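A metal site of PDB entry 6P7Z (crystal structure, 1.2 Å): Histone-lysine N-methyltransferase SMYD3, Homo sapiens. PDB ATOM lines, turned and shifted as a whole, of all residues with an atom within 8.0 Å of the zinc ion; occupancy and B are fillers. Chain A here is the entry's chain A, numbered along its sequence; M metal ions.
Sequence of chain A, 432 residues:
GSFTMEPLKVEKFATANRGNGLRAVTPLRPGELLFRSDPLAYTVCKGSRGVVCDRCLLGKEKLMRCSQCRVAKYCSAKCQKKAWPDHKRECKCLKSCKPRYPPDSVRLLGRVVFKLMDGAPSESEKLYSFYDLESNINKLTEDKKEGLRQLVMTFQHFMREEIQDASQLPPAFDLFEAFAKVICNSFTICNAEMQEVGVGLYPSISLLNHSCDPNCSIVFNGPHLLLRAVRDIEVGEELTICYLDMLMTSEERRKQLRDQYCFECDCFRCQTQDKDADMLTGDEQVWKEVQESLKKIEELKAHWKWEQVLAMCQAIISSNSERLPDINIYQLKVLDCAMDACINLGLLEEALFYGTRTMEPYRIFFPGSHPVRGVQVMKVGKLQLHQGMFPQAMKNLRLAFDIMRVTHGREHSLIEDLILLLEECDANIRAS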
ATOM      1  N   ASP A  54      -0.014  -3.226 -22.270  1.00  0.00           N
ATOM      2  CA  ASP A  54       1.364  -3.192 -21.771  1.00  0.00           C
ATOM      3  C   ASP A  54       1.429  -2.745 -20.320  1.00  0.00           C
ATOM      4  O   ASP A  54       2.288  -3.209 -19.567  1.00  0.00           O
ATOM      5  CB  ASP A  54       2.211  -2.194 -22.566  1.00  0.00           C
ATOM      6  CG  ASP A  54       2.908  -2.799 -23.775  1.00  0.00           C
ATOM      7  OD1 ASP A  54       2.289  -3.560 -24.552  1.00  0.00           O
ATOM      8  OD2 ASP A  54       4.097  -2.467 -23.959  1.00  0.00           O
ATOM      9  N   ARG A  65      -2.074   1.297 -30.223  1.00  0.00           N
ATOM     10  CA  ARG A  65      -0.635   1.108 -30.264  1.00  0.00           C
ATOM     11  C   ARG A  65       0.087   2.454 -30.138  1.00  0.00           C
ATOM     12  O   ARG A  65      -0.420   3.491 -30.550  1.00  0.00           O
ATOM     13  CB  ARG A  65      -0.210   0.429 -31.559  1.00  0.00           C
ATOM     14  CG  ARG A  65      -0.514   1.213 -32.816  1.00  0.00           C
ATOM     15  CD  ARG A  65      -0.265   0.387 -34.057  1.00  0.00           C
ATOM     16  NE  ARG A  65      -0.710   1.107 -35.246  1.00  0.00           N
ATOM     17  CZ  ARG A  65      -0.541   0.672 -36.485  1.00  0.00           C
ATOM     18  NH1 ARG A  65       0.073  -0.489 -36.706  1.00  0.00           N
ATOM     19  NH2 ARG A  65      -0.985   1.392 -37.511  1.00  0.00           N
ATOM     20  N   CYS A  66       1.267   2.399 -29.544  1.00  0.00           N
ATOM     21  CA  CYS A  66       2.175   3.539 -29.576  1.00  0.00           C
ATOM     22  C   CYS A  66       2.506   3.861 -31.017  1.00  0.00           C
ATOM     23  O   CYS A  66       2.931   2.997 -31.785  1.00  0.00           O
ATOM     24  CB  CYS A  66       3.458   3.185 -28.834  1.00  0.00           C
ATOM     25  SG  CYS A  66       4.683   4.498 -28.887  1.00  0.00           S
ATOM     26  N   SER A  67       2.296   5.114 -31.408  1.00  0.00           N
ATOM     27  CA  SER A  67       2.509   5.442 -32.812  1.00  0.00           C
ATOM     28  C   SER A  67       3.973   5.390 -33.209  1.00  0.00           C
ATOM     29  O   SER A  67       4.286   5.119 -34.373  1.00  0.00           O
ATOM     30  CB  SER A  67       1.903   6.810 -33.126  1.00  0.00           C
ATOM     31  OG  SER A  67       2.052   7.071 -34.502  1.00  0.00           O
ATOM     32  N   GLN A  68       4.880   5.668 -32.273  1.00  0.00           N
ATOM     33  CA  GLN A  68       6.299   5.735 -32.622  1.00  0.00           C
ATOM     34  C   GLN A  68       6.876   4.349 -32.894  1.00  0.00           C
ATOM     35  O   GLN A  68       7.536   4.139 -33.913  1.00  0.00           O
ATOM     36  CB  GLN A  68       7.093   6.451 -31.528  1.00  0.00           C
ATOM     37  CG  GLN A  68       8.580   6.545 -31.876  1.00  0.00           C
ATOM     38  CD  GLN A  68       9.307   7.619 -31.099  1.00  0.00           C
ATOM     39  OE1 GLN A  68       9.798   8.591 -31.678  1.00  0.00           O
ATOM     40  NE2 GLN A  68       9.408   7.453 -29.779  1.00  0.00           N
ATOM     41  N   CYS A  69       6.656   3.396 -31.993  1.00  0.00           N
ATOM     42  CA  CYS A  69       7.236   2.064 -32.161  1.00  0.00           C
ATOM     43  C   CYS A  69       6.248   1.057 -32.718  1.00  0.00           C
ATOM     44  O   CYS A  69       6.683   0.058 -33.325  1.00  0.00           O
ATOM     45  CB  CYS A  69       7.817   1.538 -30.841  1.00  0.00           C
ATOM     46  SG  CYS A  69       6.601   1.234 -29.536  1.00  0.00           S
ATOM     47  N   ARG A  70       4.949   1.270 -32.524  1.00  0.00           N
ATOM     48  CA  ARG A  70       3.896   0.335 -32.925  1.00  0.00           C
ATOM     49  C   ARG A  70       4.070  -1.047 -32.320  1.00  0.00           C
ATOM     50  O   ARG A  70       3.505  -2.026 -32.828  1.00  0.00           O
ATOM     51  CB  ARG A  70       3.716   0.281 -34.450  1.00  0.00           C
ATOM     52  CG  ARG A  70       3.199   1.588 -35.022  1.00  0.00           C
ATOM     53  CD  ARG A  70       3.092   1.533 -36.517  1.00  0.00           C
ATOM     54  NE  ARG A  70       2.254   2.605 -37.029  1.00  0.00           N
ATOM     55  CZ  ARG A  70       1.889   2.710 -38.301  1.00  0.00           C
ATOM     56  NH1 ARG A  70       2.308   1.812 -39.181  1.00  0.00           N
ATOM     57  NH2 ARG A  70       1.124   3.721 -38.688  1.00  0.00           N
ATOM     58  N   VAL A  71       4.804  -1.137 -31.221  1.00  0.00           N
ATOM     59  CA  VAL A  71       5.006  -2.391 -30.503  1.00  0.00           C
ATOM     60  C   VAL A  71       4.241  -2.397 -29.191  1.00  0.00           C
ATOM     61  O   VAL A  71       3.518  -3.342 -28.882  1.00  0.00           O
ATOM     62  CB  VAL A  71       6.509  -2.671 -30.282  1.00  0.00           C
ATOM     63  CG1 VAL A  71       6.700  -3.876 -29.381  1.00  0.00           C
ATOM     64  CG2 VAL A  71       7.218  -2.876 -31.616  1.00  0.00           C
ATOM     65  N   ALA A  72       4.409  -1.351 -28.377  1.00  0.00           N
ATOM     66  CA  ALA A  72       3.637  -1.219 -27.156  1.00  0.00           C
ATOM     67  C   ALA A  72       2.167  -0.956 -27.506  1.00  0.00           C
ATOM     68  O   ALA A  72       1.857  -0.172 -28.409  1.00  0.00           O
ATOM     69  CB  ALA A  72       4.182  -0.071 -26.314  1.00  0.00           C
ATOM     70  N   LYS A  73       1.271  -1.620 -26.766  1.00  0.00           N
ATOM     71  CA  LYS A  73      -0.152  -1.491 -27.014  1.00  0.00           C
ATOM     72  C   LYS A  73      -0.877  -1.344 -25.690  1.00  0.00           C
ATOM     73  O   LYS A  73      -0.465  -1.917 -24.677  1.00  0.00           O
ATOM     74  CB  LYS A  73      -0.694  -2.660 -27.848  1.00  0.00           C
ATOM     75  CG  LYS A  73      -0.168  -2.663 -29.286  1.00  0.00           C
ATOM     76  CD  LYS A  73      -0.622  -3.886 -30.060  1.00  0.00           C
ATOM     77  CE  LYS A  73      -0.185  -3.791 -31.518  1.00  0.00           C
ATOM     78  NZ  LYS A  73      -0.484  -5.037 -32.265  1.00  0.00           N
ATOM     79  N   TYR A  74      -1.969  -0.584 -25.690  1.00  0.00           N
ATOM     80  CA  TYR A  74      -2.592  -0.149 -24.457  1.00  0.00           C
ATOM     81  C   TYR A  74      -4.099  -0.241 -24.555  1.00  0.00           C
ATOM     82  O   TYR A  74      -4.679  -0.195 -25.647  1.00  0.00           O
ATOM     83  CB  TYR A  74      -2.183   1.287 -24.123  1.00  0.00           C
ATOM     84  CG  TYR A  74      -0.684   1.477 -24.043  1.00  0.00           C
ATOM     85  CD1 TYR A  74       0.013   1.115 -22.901  1.00  0.00           C
ATOM     86  CD2 TYR A  74       0.028   2.007 -25.113  1.00  0.00           C
ATOM     87  CE1 TYR A  74       1.382   1.296 -22.813  1.00  0.00           C
ATOM     88  CE2 TYR A  74       1.396   2.194 -25.032  1.00  0.00           C
ATOM     89  CZ  TYR A  74       2.065   1.823 -23.881  1.00  0.00           C
ATOM     90  OH  TYR A  74       3.434   2.011 -23.786  1.00  0.00           O
ATOM     91  N   GLN A  80      -1.701   4.425 -21.856  1.00  0.00           N
ATOM     92  CA  GLN A  80      -0.623   4.769 -22.778  1.00  0.00           C
ATOM     93  C   GLN A  80       0.170   5.945 -22.244  1.00  0.00           C
ATOM     94  O   GLN A  80       1.413   5.947 -22.289  1.00  0.00           O
ATOM     95  CB  GLN A  80      -1.172   5.083 -24.162  1.00  0.00           C
ATOM     96  CG  GLN A  80      -0.084   5.510 -25.145  1.00  0.00           C
ATOM     97  CD  GLN A  80      -0.538   5.580 -26.587  1.00  0.00           C
ATOM     98  OE1 GLN A  80      -1.656   5.168 -26.922  1.00  0.00           O
ATOM     99  NE2 GLN A  80       0.320   6.094 -27.445  1.00  0.00           N
ATOM    100  N   TRP A  84       4.190   6.139 -20.553  1.00  0.00           N
ATOM    101  CA  TRP A  84       5.190   6.785 -21.406  1.00  0.00           C
ATOM    102  C   TRP A  84       6.539   6.959 -20.734  1.00  0.00           C
ATOM    103  O   TRP A  84       7.551   6.579 -21.342  1.00  0.00           O
ATOM    104  CB  TRP A  84       4.641   8.074 -22.004  1.00  0.00           C
ATOM    105  CG  TRP A  84       5.659   8.809 -22.790  1.00  0.00           C
ATOM    106  CD1 TRP A  84       6.222  10.022 -22.492  1.00  0.00           C
ATOM    107  CD2 TRP A  84       6.271   8.381 -24.016  1.00  0.00           C
ATOM    108  NE1 TRP A  84       7.137  10.366 -23.445  1.00  0.00           N
ATOM    109  CE2 TRP A  84       7.186   9.380 -24.397  1.00  0.00           C
ATOM    110  CE3 TRP A  84       6.130   7.251 -24.828  1.00  0.00           C
ATOM    111  CZ2 TRP A  84       7.949   9.278 -25.562  1.00  0.00           C
ATOM    112  CZ3 TRP A  84       6.884   7.157 -25.972  1.00  0.00           C
ATOM    113  CH2 TRP A  84       7.789   8.163 -26.331  1.00  0.00           C
ATOM    114  N   HIS A  87       8.342   3.769 -20.904  1.00  0.00           N
ATOM    115  CA  HIS A  87       8.410   3.251 -22.261  1.00  0.00           C
ATOM    116  C   HIS A  87       9.279   4.097 -23.185  1.00  0.00           C
ATOM    117  O   HIS A  87       9.729   3.592 -24.226  1.00  0.00           O
ATOM    118  CB  HIS A  87       6.983   3.125 -22.837  1.00  0.00           C
ATOM    119  CG  HIS A  87       6.950   2.779 -24.295  1.00  0.00           C
ATOM    120  ND1 HIS A  87       7.417   1.588 -24.796  1.00  0.00           N
ATOM    121  CD2 HIS A  87       6.503   3.489 -25.369  1.00  0.00           C
ATOM    122  CE1 HIS A  87       7.268   1.580 -26.119  1.00  0.00           C
ATOM    123  NE2 HIS A  87       6.716   2.722 -26.483  1.00  0.00           N
ATOM    124  N   LYS A  88       9.554   5.340 -22.805  1.00  0.00           N
ATOM    125  CA  LYS A  88      10.112   6.325 -23.737  1.00  0.00           C
ATOM    126  C   LYS A  88      11.431   5.862 -24.354  1.00  0.00           C
ATOM    127  O   LYS A  88      11.641   5.986 -25.564  1.00  0.00           O
ATOM    128  CB  LYS A  88      10.282   7.659 -23.014  1.00  0.00           C
ATOM    129  CG  LYS A  88      11.078   8.697 -23.779  1.00  0.00           C
ATOM    130  CD  LYS A  88      11.282   9.954 -22.941  1.00  0.00           C
ATOM    131  N   ARG A  89      12.349   5.349 -23.531  1.00  0.00           N
ATOM    132  CA  ARG A  89      13.657   4.981 -24.059  1.00  0.00           C
ATOM    133  C   ARG A  89      13.614   3.662 -24.812  1.00  0.00           C
ATOM    134  O   ARG A  89      14.247   3.527 -25.854  1.00  0.00           O
ATOM    135  CB  ARG A  89      14.707   4.979 -22.949  1.00  0.00           C
ATOM    136  CG  ARG A  89      14.905   6.367 -22.358  1.00  0.00           C
ATOM    137  CD  ARG A  89      16.034   6.431 -21.348  1.00  0.00           C
ATOM    138  NE  ARG A  89      17.338   6.180 -21.960  1.00  0.00           N
ATOM    139  CZ  ARG A  89      18.461   6.017 -21.280  1.00  0.00           C
ATOM    140  NH1 ARG A  89      18.436   6.076 -19.954  1.00  0.00           N
ATOM    141  NH2 ARG A  89      19.602   5.789 -21.903  1.00  0.00           N
ATOM    142  N   GLU A  90      12.856   2.680 -24.315  1.00  0.00           N
ATOM    143  CA  GLU A  90      12.738   1.434 -25.059  1.00  0.00           C
ATOM    144  C   GLU A  90      12.010   1.644 -26.377  1.00  0.00           C
ATOM    145  O   GLU A  90      12.249   0.921 -27.345  1.00  0.00           O
ATOM    146  CB  GLU A  90      12.061   0.344 -24.222  1.00  0.00           C
ATOM    147  CG  GLU A  90      10.556   0.478 -24.181  1.00  0.00           C
ATOM    148  CD  GLU A  90       9.809  -0.728 -23.631  1.00  0.00           C
ATOM    149  OE1 GLU A  90      10.404  -1.782 -23.274  1.00  0.00           O
ATOM    150  OE2 GLU A  90       8.568  -0.609 -23.571  1.00  0.00           O
ATOM    151  N   CYS A  91      11.146   2.668 -26.439  1.00  0.00           N
ATOM    152  CA  CYS A  91      10.400   2.938 -27.658  1.00  0.00           C
ATOM    153  C   CYS A  91      11.358   3.191 -28.824  1.00  0.00           C
ATOM    154  O   CYS A  91      11.196   2.624 -29.908  1.00  0.00           O
ATOM    155  CB  CYS A  91       9.499   4.161 -27.450  1.00  0.00           C
ATOM    156  SG  CYS A  91       8.468   4.586 -28.858  1.00  0.00           S
ATOM    157  N   LYS A  92      12.365   4.038 -28.594  1.00  0.00           N
ATOM    158  CA  LYS A  92      13.349   4.327 -29.634  1.00  0.00           C
ATOM    159  C   LYS A  92      14.118   3.071 -30.045  1.00  0.00           C
ATOM    160  O   LYS A  92      14.492   2.925 -31.212  1.00  0.00           O
ATOM    161  CB  LYS A  92      14.316   5.408 -29.157  1.00  0.00           C
ATOM    162  CG  LYS A  92      13.697   6.798 -29.053  1.00  0.00           C
ATOM    163  N   CYS A  93      14.341   2.154 -29.103  1.00  0.00           N
ATOM    164  CA  CYS A  93      15.053   0.918 -29.433  1.00  0.00           C
ATOM    165  C   CYS A  93      14.159  -0.048 -30.197  1.00  0.00           C
ATOM    166  O   CYS A  93      14.601  -0.664 -31.176  1.00  0.00           O
ATOM    167  CB  CYS A  93      15.560   0.263 -28.152  1.00  0.00           C
ATOM    168  SG  CYS A  93      16.676   1.268 -27.191  1.00  0.00           S
ATOM    169  N   LEU A  94      12.902  -0.192 -29.777  1.00  0.00           N
ATOM    170  CA  LEU A  94      11.979  -1.106 -30.449  1.00  0.00           C
ATOM    171  C   LEU A  94      11.708  -0.653 -31.878  1.00  0.00           C
ATOM    172  O   LEU A  94      11.587  -1.473 -32.790  1.00  0.00           O
ATOM    173  CB  LEU A  94      10.686  -1.231 -29.651  1.00  0.00           C
ATOM    174  CG  LEU A  94      10.740  -1.945 -28.296  1.00  0.00           C
ATOM    175  CD1 LEU A  94       9.515  -1.601 -27.459  1.00  0.00           C
ATOM    176  CD2 LEU A  94      10.837  -3.444 -28.510  1.00  0.00           C
ATOM    177  N   LYS A  95      11.596   0.665 -32.086  1.00  0.00           N
ATOM    178  CA  LYS A  95      11.406   1.184 -33.438  1.00  0.00           C
ATOM    179  C   LYS A  95      12.607   0.865 -34.317  1.00  0.00           C
ATOM    180  O   LYS A  95      12.438   0.458 -35.472  1.00  0.00           O
ATOM    181  CB  LYS A  95      11.178   2.695 -33.372  1.00  0.00           C
ATOM    182  N   ARG A 107      13.988  -7.315 -23.175  1.00  0.00           N
ATOM    183  CA  ARG A 107      13.121  -6.153 -22.973  1.00  0.00           C
ATOM    184  C   ARG A 107      13.016  -5.831 -21.492  1.00  0.00           C
ATOM    185  O   ARG A 107      13.047  -4.656 -21.086  1.00  0.00           O
ATOM    186  CB  ARG A 107      11.741  -6.398 -23.583  1.00  0.00           C
ATOM    187  CG  ARG A 107      10.866  -5.166 -23.575  1.00  0.00           C
ATOM    188  CD  ARG A 107       9.582  -5.346 -24.343  1.00  0.00           C
ATOM    189  NE  ARG A 107       8.807  -4.106 -24.328  1.00  0.00           N
ATOM    190  CZ  ARG A 107       7.553  -3.986 -24.757  1.00  0.00           C
ATOM    191  NH1 ARG A 107       6.925  -5.040 -25.243  1.00  0.00           N
ATOM    192  NH2 ARG A 107       6.927  -2.811 -24.699  1.00  0.00           N
HETATM  193 ZN    ZN M   1       6.603   3.288 -28.431  1.00  0.00          ZN
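NE2 of His 87 binds the zinc ion. The zinc ion is bound by the side-chain sulfur (SG) of Cys 91, at 2.3 Å. SG of Cys 66 binds the zinc ion, 2.3 Å away. The zinc ion is bound by SG of Cys 69 (2.3 Å). The zinc ion has four donor atoms within binding distance.
ND1 of His 87 is in hydrogen-bond range of OE2 of Glu 90 (2.8 Å). The backbone NH of Gln 68 sits close to the side-chain sulfur of Cys 66. The side-chain sulfur (SG) of Cys 91 sits close to the side-chain amide nitrogen (NE2) of Gln 68 (3.2 Å). The side-chain sulfur of Cys 69 lies close to the backbone NH of Ala 72, at 3.6 Å. The side-chain sulfur (SG) of Cys 69 sits close to the backbone NH (N) of Val 71 (3.4 Å). The backbone carbonyl oxygen (O) of Ala 72 is in hydrogen-bond range of the backbone NH (N) of Cys 66.
Of the 23 residues printed, 4 come within 4 Å of the zinc ion.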
